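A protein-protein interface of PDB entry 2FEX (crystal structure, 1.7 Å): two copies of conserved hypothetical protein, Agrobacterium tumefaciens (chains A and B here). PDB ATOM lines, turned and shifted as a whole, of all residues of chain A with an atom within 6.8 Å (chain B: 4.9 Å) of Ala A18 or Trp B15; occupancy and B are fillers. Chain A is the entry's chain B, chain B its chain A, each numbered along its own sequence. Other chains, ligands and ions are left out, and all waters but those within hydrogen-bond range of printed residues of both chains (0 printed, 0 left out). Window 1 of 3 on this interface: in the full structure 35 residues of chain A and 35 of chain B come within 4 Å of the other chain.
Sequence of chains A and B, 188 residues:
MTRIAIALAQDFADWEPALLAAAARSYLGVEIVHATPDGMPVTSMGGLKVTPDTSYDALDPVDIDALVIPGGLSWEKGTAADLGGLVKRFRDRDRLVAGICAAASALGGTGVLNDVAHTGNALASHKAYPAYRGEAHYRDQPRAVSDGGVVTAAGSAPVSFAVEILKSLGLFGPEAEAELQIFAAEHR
Of chain A, only Ala A18, Ala A22, Tyr A27 and Phe A183 come within 4 Å of Trp B15.
Of the printed residues of chain B, Asp A14 touches Ala B18.
Of the printed residues of chain A, Pro B158 touches Phe A183.
Printed residues of chain A within 4 Å of Gly B155: Phe A183.
Of the printed residues of chain B, Ala A22 touches Asp B14, Trp B15 and Met B45.
Of the printed residues of chain B, Phe A183 touches Trp B15, Gly B155 and Pro B158.
The nearest residue of chain B that does not touch Ala A18 is Ala B18 (4.6 Å).
The nearest residue of chain A that does not touch Trp B15 is Leu A19 (4.1 Å).
Asp A14 touches Ala B18, and with the chains exchanged Ala A18 touches Asp B14.
Trp A15 touches Ala B18, and with the chains exchanged Ala A18 touches Trp B15.
7 positions are printed for both chains.
The side-chain carboxylate of Glu A16 sits close to the indole nitrogen of Trp A15.
NE1 of Trp B15 sits at hydrogen-bond distance from O of Gly B155, 2.9 Å away.
OD2 of Asp B14 lies within hydrogen-bond range of N of Met B45.
NE1 of Trp B15 lies close to OE2 of Glu B16 (3.5 Å).
Of the 18 printed residues of chain A, 6 touch a printed residue of chain B.
Hydrophobic or aromatic side chains of chain A that line the printed part of chain B: Ala A18, Ala A22, Tyr A27 and Phe A183.
Among the printed residues, pairs that only touch across the chains: Asp A14 with Ala B18 (3.6 Å), Trp A15 with Ala B18 (3.7 Å), Ala A18 with Asp B14 (3.6 Å), Ala A18 with Trp B15 (3.6 Å), Ala A22 with Asp B14 (3.5 Å), Ala A22 with Trp B15 (3.5 Å), Ala A22 with Met B45 (3.8 Å), Tyr A27 with Trp B15 (3.7 Å), Tyr A27 with Met B45 (3.6 Å), Phe A183 with Trp B15 (3.6 Å), Phe A183 with Gly B155 (3.6 Å) and Phe A183 with Pro B158 (3.9 Å).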
ATOM      1  N   ILE A   6      31.807   4.600 -37.914  1.00  0.00           N
ATOM      2  CA  ILE A   6      32.202   5.145 -36.615  1.00  0.00           C
ATOM      3  C   ILE A   6      33.728   5.284 -36.636  1.00  0.00           C
ATOM      4  O   ILE A   6      34.464   4.284 -36.800  1.00  0.00           O
ATOM      5  CB  ILE A   6      31.693   4.234 -35.470  1.00  0.00           C
ATOM      6  CG1 ILE A   6      30.141   4.292 -35.475  1.00  0.00           C
ATOM      7  CG2 ILE A   6      32.260   4.777 -34.123  1.00  0.00           C
ATOM      8  CD1 ILE A   6      29.486   3.477 -34.356  1.00  0.00           C
ATOM      9  N   ALA A  13      36.710   7.377 -26.355  1.00  0.00           N
ATOM     10  CA  ALA A  13      35.864   7.380 -25.144  1.00  0.00           C
ATOM     11  C   ALA A  13      34.811   6.256 -25.258  1.00  0.00           C
ATOM     12  O   ALA A  13      33.875   6.347 -26.028  1.00  0.00           O
ATOM     13  CB  ALA A  13      35.219   8.786 -24.939  1.00  0.00           C
ATOM     14  N   ASP A  14      35.015   5.188 -24.493  1.00  0.00           N
ATOM     15  CA  ASP A  14      34.224   3.975 -24.718  1.00  0.00           C
ATOM     16  C   ASP A  14      32.714   4.267 -24.679  1.00  0.00           C
ATOM     17  O   ASP A  14      31.954   3.620 -25.384  1.00  0.00           O
ATOM     18  CB  ASP A  14      34.483   2.911 -23.638  1.00  0.00           C
ATOM     19  CG  ASP A  14      35.965   2.480 -23.549  1.00  0.00           C
ATOM     20  OD1 ASP A  14      36.813   3.402 -23.456  1.00  0.00           O
ATOM     21  OD2 ASP A  14      36.245   1.248 -23.571  1.00  0.00           O
ATOM     22  N   TRP A  15      32.300   5.154 -23.776  1.00  0.00           N
ATOM     23  CA  TRP A  15      30.880   5.345 -23.537  1.00  0.00           C
ATOM     24  C   TRP A  15      30.194   6.207 -24.617  1.00  0.00           C
ATOM     25  O   TRP A  15      28.951   6.335 -24.584  1.00  0.00           O
ATOM     26  CB  TRP A  15      30.616   5.976 -22.165  1.00  0.00           C
ATOM     27  CG  TRP A  15      31.071   7.442 -22.059  1.00  0.00           C
ATOM     28  CD1 TRP A  15      30.285   8.543 -22.298  1.00  0.00           C
ATOM     29  CD2 TRP A  15      32.399   7.935 -21.783  1.00  0.00           C
ATOM     30  NE1 TRP A  15      31.050   9.721 -22.167  1.00  0.00           N
ATOM     31  CE2 TRP A  15      32.344   9.362 -21.859  1.00  0.00           C
ATOM     32  CE3 TRP A  15      33.616   7.319 -21.454  1.00  0.00           C
ATOM     33  CZ2 TRP A  15      33.477  10.157 -21.628  1.00  0.00           C
ATOM     34  CZ3 TRP A  15      34.749   8.125 -21.225  1.00  0.00           C
ATOM     35  CH2 TRP A  15      34.653   9.524 -21.285  1.00  0.00           C
ATOM     36  N   GLU A  16      30.985   6.806 -25.515  1.00  0.00           N
ATOM     37  CA  GLU A  16      30.404   7.827 -26.425  1.00  0.00           C
ATOM     38  C   GLU A  16      29.688   7.235 -27.651  1.00  0.00           C
ATOM     39  O   GLU A  16      28.621   7.724 -28.021  1.00  0.00           O
ATOM     40  CB  GLU A  16      31.446   8.887 -26.767  1.00  0.00           C
ATOM     41  CG  GLU A  16      31.714   9.698 -25.472  1.00  0.00           C
ATOM     42  CD  GLU A  16      32.724  10.838 -25.564  1.00  0.00           C
ATOM     43  OE1 GLU A  16      33.295  11.018 -26.662  1.00  0.00           O
ATOM     44  OE2 GLU A  16      32.955  11.449 -24.493  1.00  0.00           O
ATOM     45  N   PRO A  17      30.269   6.226 -28.313  1.00  0.00           N
ATOM     46  CA  PRO A  17      29.585   5.649 -29.457  1.00  0.00           C
ATOM     47  C   PRO A  17      28.818   4.362 -29.118  1.00  0.00           C
ATOM     48  O   PRO A  17      28.162   3.793 -30.005  1.00  0.00           O
ATOM     49  CB  PRO A  17      30.756   5.351 -30.381  1.00  0.00           C
ATOM     50  CG  PRO A  17      31.825   4.801 -29.447  1.00  0.00           C
ATOM     51  CD  PRO A  17      31.654   5.710 -28.196  1.00  0.00           C
ATOM     52  N   ALA A  18      28.873   3.948 -27.850  1.00  0.00           N
ATOM     53  CA  ALA A  18      28.402   2.601 -27.473  1.00  0.00           C
ATOM     54  C   ALA A  18      26.919   2.354 -27.651  1.00  0.00           C
ATOM     55  O   ALA A  18      26.485   1.323 -28.220  1.00  0.00           O
ATOM     56  CB  ALA A  18      28.758   2.365 -25.964  1.00  0.00           C
ATOM     57  N   LEU A  19      26.112   3.248 -27.061  1.00  0.00           N
ATOM     58  CA  LEU A  19      24.667   3.017 -27.141  1.00  0.00           C
ATOM     59  C   LEU A  19      24.188   3.178 -28.608  1.00  0.00           C
ATOM     60  O   LEU A  19      23.378   2.371 -29.065  1.00  0.00           O
ATOM     61  CB  LEU A  19      23.938   4.052 -26.252  1.00  0.00           C
ATOM     62  CG  LEU A  19      22.446   3.894 -26.251  1.00  0.00           C
ATOM     63  CD1 LEU A  19      22.051   2.518 -25.743  1.00  0.00           C
ATOM     64  CD2 LEU A  19      21.810   4.952 -25.350  1.00  0.00           C
ATOM     65  N   LEU A  20      24.674   4.178 -29.321  1.00  0.00           N
ATOM     66  CA  LEU A  20      24.316   4.305 -30.702  1.00  0.00           C
ATOM     67  C   LEU A  20      24.631   3.035 -31.504  1.00  0.00           C
ATOM     68  O   LEU A  20      23.762   2.520 -32.179  1.00  0.00           O
ATOM     69  CB  LEU A  20      24.972   5.516 -31.343  1.00  0.00           C
ATOM     70  CG  LEU A  20      24.836   5.492 -32.850  1.00  0.00           C
ATOM     71  CD1 LEU A  20      23.436   5.843 -33.267  1.00  0.00           C
ATOM     72  CD2 LEU A  20      25.832   6.357 -33.480  1.00  0.00           C
ATOM     73  N   ALA A  21      25.865   2.549 -31.406  1.00  0.00           N
ATOM     74  CA  ALA A  21      26.247   1.399 -32.228  1.00  0.00           C
ATOM     75  C   ALA A  21      25.466   0.132 -31.831  1.00  0.00           C
ATOM     76  O   ALA A  21      24.960  -0.588 -32.706  1.00  0.00           O
ATOM     77  CB  ALA A  21      27.792   1.167 -32.061  1.00  0.00           C
ATOM     78  N   ALA A  22      25.358  -0.122 -30.516  1.00  0.00           N
ATOM     79  CA  ALA A  22      24.719  -1.332 -30.046  1.00  0.00           C
ATOM     80  C   ALA A  22      23.230  -1.326 -30.429  1.00  0.00           C
ATOM     81  O   ALA A  22      22.718  -2.340 -30.898  1.00  0.00           O
ATOM     82  CB  ALA A  22      24.873  -1.512 -28.510  1.00  0.00           C
ATOM     83  N   ALA A  23      22.558  -0.203 -30.205  1.00  0.00           N
ATOM     84  CA  ALA A  23      21.092  -0.166 -30.517  1.00  0.00           C
ATOM     85  C   ALA A  23      20.856  -0.228 -32.037  1.00  0.00           C
ATOM     86  O   ALA A  23      19.995  -0.972 -32.505  1.00  0.00           O
ATOM     87  CB  ALA A  23      20.444   1.120 -29.924  1.00  0.00           C
ATOM     88  N   ALA A  24      21.592   0.602 -32.790  1.00  0.00           N
ATOM     89  CA  ALA A  24      21.483   0.631 -34.261  1.00  0.00           C
ATOM     90  C   ALA A  24      21.693  -0.761 -34.856  1.00  0.00           C
ATOM     91  O   ALA A  24      20.856  -1.264 -35.637  1.00  0.00           O
ATOM     92  CB  ALA A  24      22.466   1.640 -34.873  1.00  0.00           C
ATOM     93  N   TYR A  27      19.406  -3.792 -32.712  1.00  0.00           N
ATOM     94  CA  TYR A  27      17.949  -3.631 -32.630  1.00  0.00           C
ATOM     95  C   TYR A  27      17.343  -3.069 -33.921  1.00  0.00           C
ATOM     96  O   TYR A  27      16.180  -3.396 -34.273  1.00  0.00           O
ATOM     97  CB  TYR A  27      17.534  -2.779 -31.399  1.00  0.00           C
ATOM     98  CG  TYR A  27      18.026  -3.154 -29.969  1.00  0.00           C
ATOM     99  CD1 TYR A  27      18.000  -4.454 -29.490  1.00  0.00           C
ATOM    100  CD2 TYR A  27      18.412  -2.138 -29.064  1.00  0.00           C
ATOM    101  CE1 TYR A  27      18.404  -4.755 -28.162  1.00  0.00           C
ATOM    102  CE2 TYR A  27      18.799  -2.420 -27.733  1.00  0.00           C
ATOM    103  CZ  TYR A  27      18.789  -3.735 -27.288  1.00  0.00           C
ATOM    104  OH  TYR A  27      19.171  -4.039 -25.966  1.00  0.00           O
ATOM    105  N   PRO A 158      25.746  11.178 -24.065  1.00  0.00           N
ATOM    106  CA  PRO A 158      25.799  10.058 -25.061  1.00  0.00           C
ATOM    107  C   PRO A 158      24.391   9.607 -25.477  1.00  0.00           C
ATOM    108  O   PRO A 158      24.207   9.126 -26.607  1.00  0.00           O
ATOM    109  CB  PRO A 158      26.531   8.889 -24.279  1.00  0.00           C
ATOM    110  CG  PRO A 158      26.192   9.164 -22.864  1.00  0.00           C
ATOM    111  CD  PRO A 158      26.281  10.770 -22.751  1.00  0.00           C
ATOM    112  N   GLU A 179      13.981   1.494 -26.802  1.00  0.00           N
ATOM    113  CA  GLU A 179      15.301   1.066 -26.328  1.00  0.00           C
ATOM    114  C   GLU A 179      16.107   2.232 -25.728  1.00  0.00           C
ATOM    115  O   GLU A 179      16.962   1.987 -24.863  1.00  0.00           O
ATOM    116  CB  GLU A 179      16.138   0.434 -27.438  1.00  0.00           C
ATOM    117  CG  GLU A 179      15.513  -0.797 -28.086  1.00  0.00           C
ATOM    118  CD  GLU A 179      15.386  -1.972 -27.132  1.00  0.00           C
ATOM    119  OE1 GLU A 179      16.082  -2.014 -26.086  1.00  0.00           O
ATOM    120  OE2 GLU A 179      14.576  -2.863 -27.457  1.00  0.00           O
ATOM    121  N   ILE A 182      15.178   4.615 -21.746  1.00  0.00           N
ATOM    122  CA  ILE A 182      15.223   3.902 -20.444  1.00  0.00           C
ATOM    123  C   ILE A 182      16.291   4.495 -19.510  1.00  0.00           C
ATOM    124  O   ILE A 182      16.331   4.168 -18.328  1.00  0.00           O
ATOM    125  CB  ILE A 182      15.481   2.399 -20.659  1.00  0.00           C
ATOM    126  CG1 ILE A 182      16.857   2.115 -21.314  1.00  0.00           C
ATOM    127  CG2 ILE A 182      14.357   1.782 -21.504  1.00  0.00           C
ATOM    128  CD1 ILE A 182      17.229   0.573 -21.429  1.00  0.00           C
ATOM    129  N   PHE A 183      17.172   5.308 -20.085  1.00  0.00           N
ATOM    130  CA  PHE A 183      18.400   5.805 -19.389  1.00  0.00           C
ATOM    131  C   PHE A 183      18.228   6.965 -18.434  1.00  0.00           C
ATOM    132  O   PHE A 183      19.121   7.279 -17.635  1.00  0.00           O
ATOM    133  CB  PHE A 183      19.497   6.065 -20.427  1.00  0.00           C
ATOM    134  CG  PHE A 183      19.914   4.808 -21.106  1.00  0.00           C
ATOM    135  CD1 PHE A 183      20.775   3.901 -20.417  1.00  0.00           C
ATOM    136  CD2 PHE A 183      19.394   4.446 -22.347  1.00  0.00           C
ATOM    137  CE1 PHE A 183      21.171   2.686 -21.025  1.00  0.00           C
ATOM    138  CE2 PHE A 183      19.737   3.222 -22.937  1.00  0.00           C
ATOM    139  CZ  PHE A 183      20.655   2.337 -22.256  1.00  0.00           C
ATOM    140  N   ALA B  13      26.905  -6.017 -24.314  1.00  0.00           N
ATOM    141  CA  ALA B  13      26.237  -4.711 -24.434  1.00  0.00           C
ATOM    142  C   ALA B  13      27.305  -3.605 -24.299  1.00  0.00           C
ATOM    143  O   ALA B  13      27.841  -3.353 -23.219  1.00  0.00           O
ATOM    144  CB  ALA B  13      25.154  -4.577 -23.319  1.00  0.00           C
ATOM    145  N   ASP B  14      27.604  -2.931 -25.414  1.00  0.00           N
ATOM    146  CA  ASP B  14      28.734  -1.957 -25.434  1.00  0.00           C
ATOM    147  C   ASP B  14      28.611  -0.917 -24.343  1.00  0.00           C
ATOM    148  O   ASP B  14      29.626  -0.474 -23.796  1.00  0.00           O
ATOM    149  CB  ASP B  14      28.797  -1.178 -26.754  1.00  0.00           C
ATOM    150  CG  ASP B  14      28.868  -2.089 -27.980  1.00  0.00           C
ATOM    151  OD1 ASP B  14      29.769  -1.830 -28.843  1.00  0.00           O
ATOM    152  OD2 ASP B  14      28.033  -3.004 -28.110  1.00  0.00           O
ATOM    153  N   TRP B  15      27.368  -0.474 -24.050  1.00  0.00           N
ATOM    154  CA  TRP B  15      27.208   0.689 -23.144  1.00  0.00           C
ATOM    155  C   TRP B  15      27.337   0.289 -21.652  1.00  0.00           C
ATOM    156  O   TRP B  15      27.320   1.164 -20.780  1.00  0.00           O
ATOM    157  CB  TRP B  15      25.840   1.343 -23.356  1.00  0.00           C
ATOM    158  CG  TRP B  15      24.685   0.522 -22.900  1.00  0.00           C
ATOM    159  CD1 TRP B  15      24.069   0.588 -21.667  1.00  0.00           C
ATOM    160  CD2 TRP B  15      23.962  -0.430 -23.672  1.00  0.00           C
ATOM    161  NE1 TRP B  15      23.014  -0.327 -21.617  1.00  0.00           N
ATOM    162  CE2 TRP B  15      22.931  -0.967 -22.826  1.00  0.00           C
ATOM    163  CE3 TRP B  15      24.095  -0.936 -24.967  1.00  0.00           C
ATOM    164  CZ2 TRP B  15      22.057  -1.970 -23.265  1.00  0.00           C
ATOM    165  CZ3 TRP B  15      23.213  -1.950 -25.404  1.00  0.00           C
ATOM    166  CH2 TRP B  15      22.183  -2.424 -24.557  1.00  0.00           C
ATOM    167  N   GLU B  16      27.451  -1.018 -21.345  1.00  0.00           N
ATOM    168  CA  GLU B  16      27.311  -1.442 -19.967  1.00  0.00           C
ATOM    169  C   GLU B  16      28.617  -1.383 -19.155  1.00  0.00           C
ATOM    170  O   GLU B  16      28.567  -1.022 -17.979  1.00  0.00           O
ATOM    171  CB  GLU B  16      26.615  -2.824 -19.905  1.00  0.00           C
ATOM    172  CG  GLU B  16      25.143  -2.601 -20.352  1.00  0.00           C
ATOM    173  CD  GLU B  16      24.221  -3.824 -20.329  1.00  0.00           C
ATOM    174  OE1 GLU B  16      24.686  -4.906 -19.996  1.00  0.00           O
ATOM    175  OE2 GLU B  16      23.001  -3.647 -20.641  1.00  0.00           O
ATOM    176  N   PRO B  17      29.762  -1.773 -19.752  1.00  0.00           N
ATOM    177  CA  PRO B  17      31.002  -1.657 -18.978  1.00  0.00           C
ATOM    178  C   PRO B  17      31.850  -0.467 -19.388  1.00  0.00           C
ATOM    179  O   PRO B  17      32.969  -0.305 -18.884  1.00  0.00           O
ATOM    180  CB  PRO B  17      31.717  -2.962 -19.349  1.00  0.00           C
ATOM    181  CG  PRO B  17      31.427  -3.120 -20.808  1.00  0.00           C
ATOM    182  CD  PRO B  17      29.973  -2.532 -21.008  1.00  0.00           C
ATOM    183  N   ALA B  18      31.319   0.354 -20.306  1.00  0.00           N
ATOM    184  CA  ALA B  18      32.136   1.372 -20.947  1.00  0.00           C
ATOM    185  C   ALA B  18      32.584   2.519 -20.054  1.00  0.00           C
ATOM    186  O   ALA B  18      33.778   2.887 -19.985  1.00  0.00           O
ATOM    187  CB  ALA B  18      31.312   1.968 -22.173  1.00  0.00           C
ATOM    188  N   MET B  45      27.674  -5.993 -29.265  1.00  0.00           N
ATOM    189  CA  MET B  45      26.394  -5.711 -29.941  1.00  0.00           C
ATOM    190  C   MET B  45      26.563  -4.640 -31.019  1.00  0.00           C
ATOM    191  O   MET B  45      25.874  -4.685 -32.044  1.00  0.00           O
ATOM    192  CB  MET B  45      25.328  -5.249 -28.923  1.00  0.00           C
ATOM    193  CG  MET B  45      24.693  -6.442 -28.243  1.00  0.00           C
ATOM    194  SD  MET B  45      23.563  -5.852 -26.734  1.00  0.00           S
ATOM    195  CE  MET B  45      22.077  -5.003 -27.801  1.00  0.00           C
ATOM    196  N   GLY B 155      20.200  -2.993 -17.200  1.00  0.00           N
ATOM    197  CA  GLY B 155      20.937  -2.454 -18.335  1.00  0.00           C
ATOM    198  C   GLY B 155      20.719  -0.955 -18.512  1.00  0.00           C
ATOM    199  O   GLY B 155      21.567  -0.287 -19.098  1.00  0.00           O
ATOM    200  N   PRO B 158      23.739   2.145 -16.378  1.00  0.00           N
ATOM    201  CA  PRO B 158      25.194   1.999 -16.453  1.00  0.00           C
ATOM    202  C   PRO B 158      25.966   2.955 -15.542  1.00  0.00           C
ATOM    203  O   PRO B 158      27.087   2.631 -15.120  1.00  0.00           O
ATOM    204  CB  PRO B 158      25.500   2.285 -17.944  1.00  0.00           C
ATOM    205  CG  PRO B 158      24.387   3.231 -18.406  1.00  0.00           C
ATOM    206  CD  PRO B 158      23.162   2.684 -17.640  1.00  0.00           C
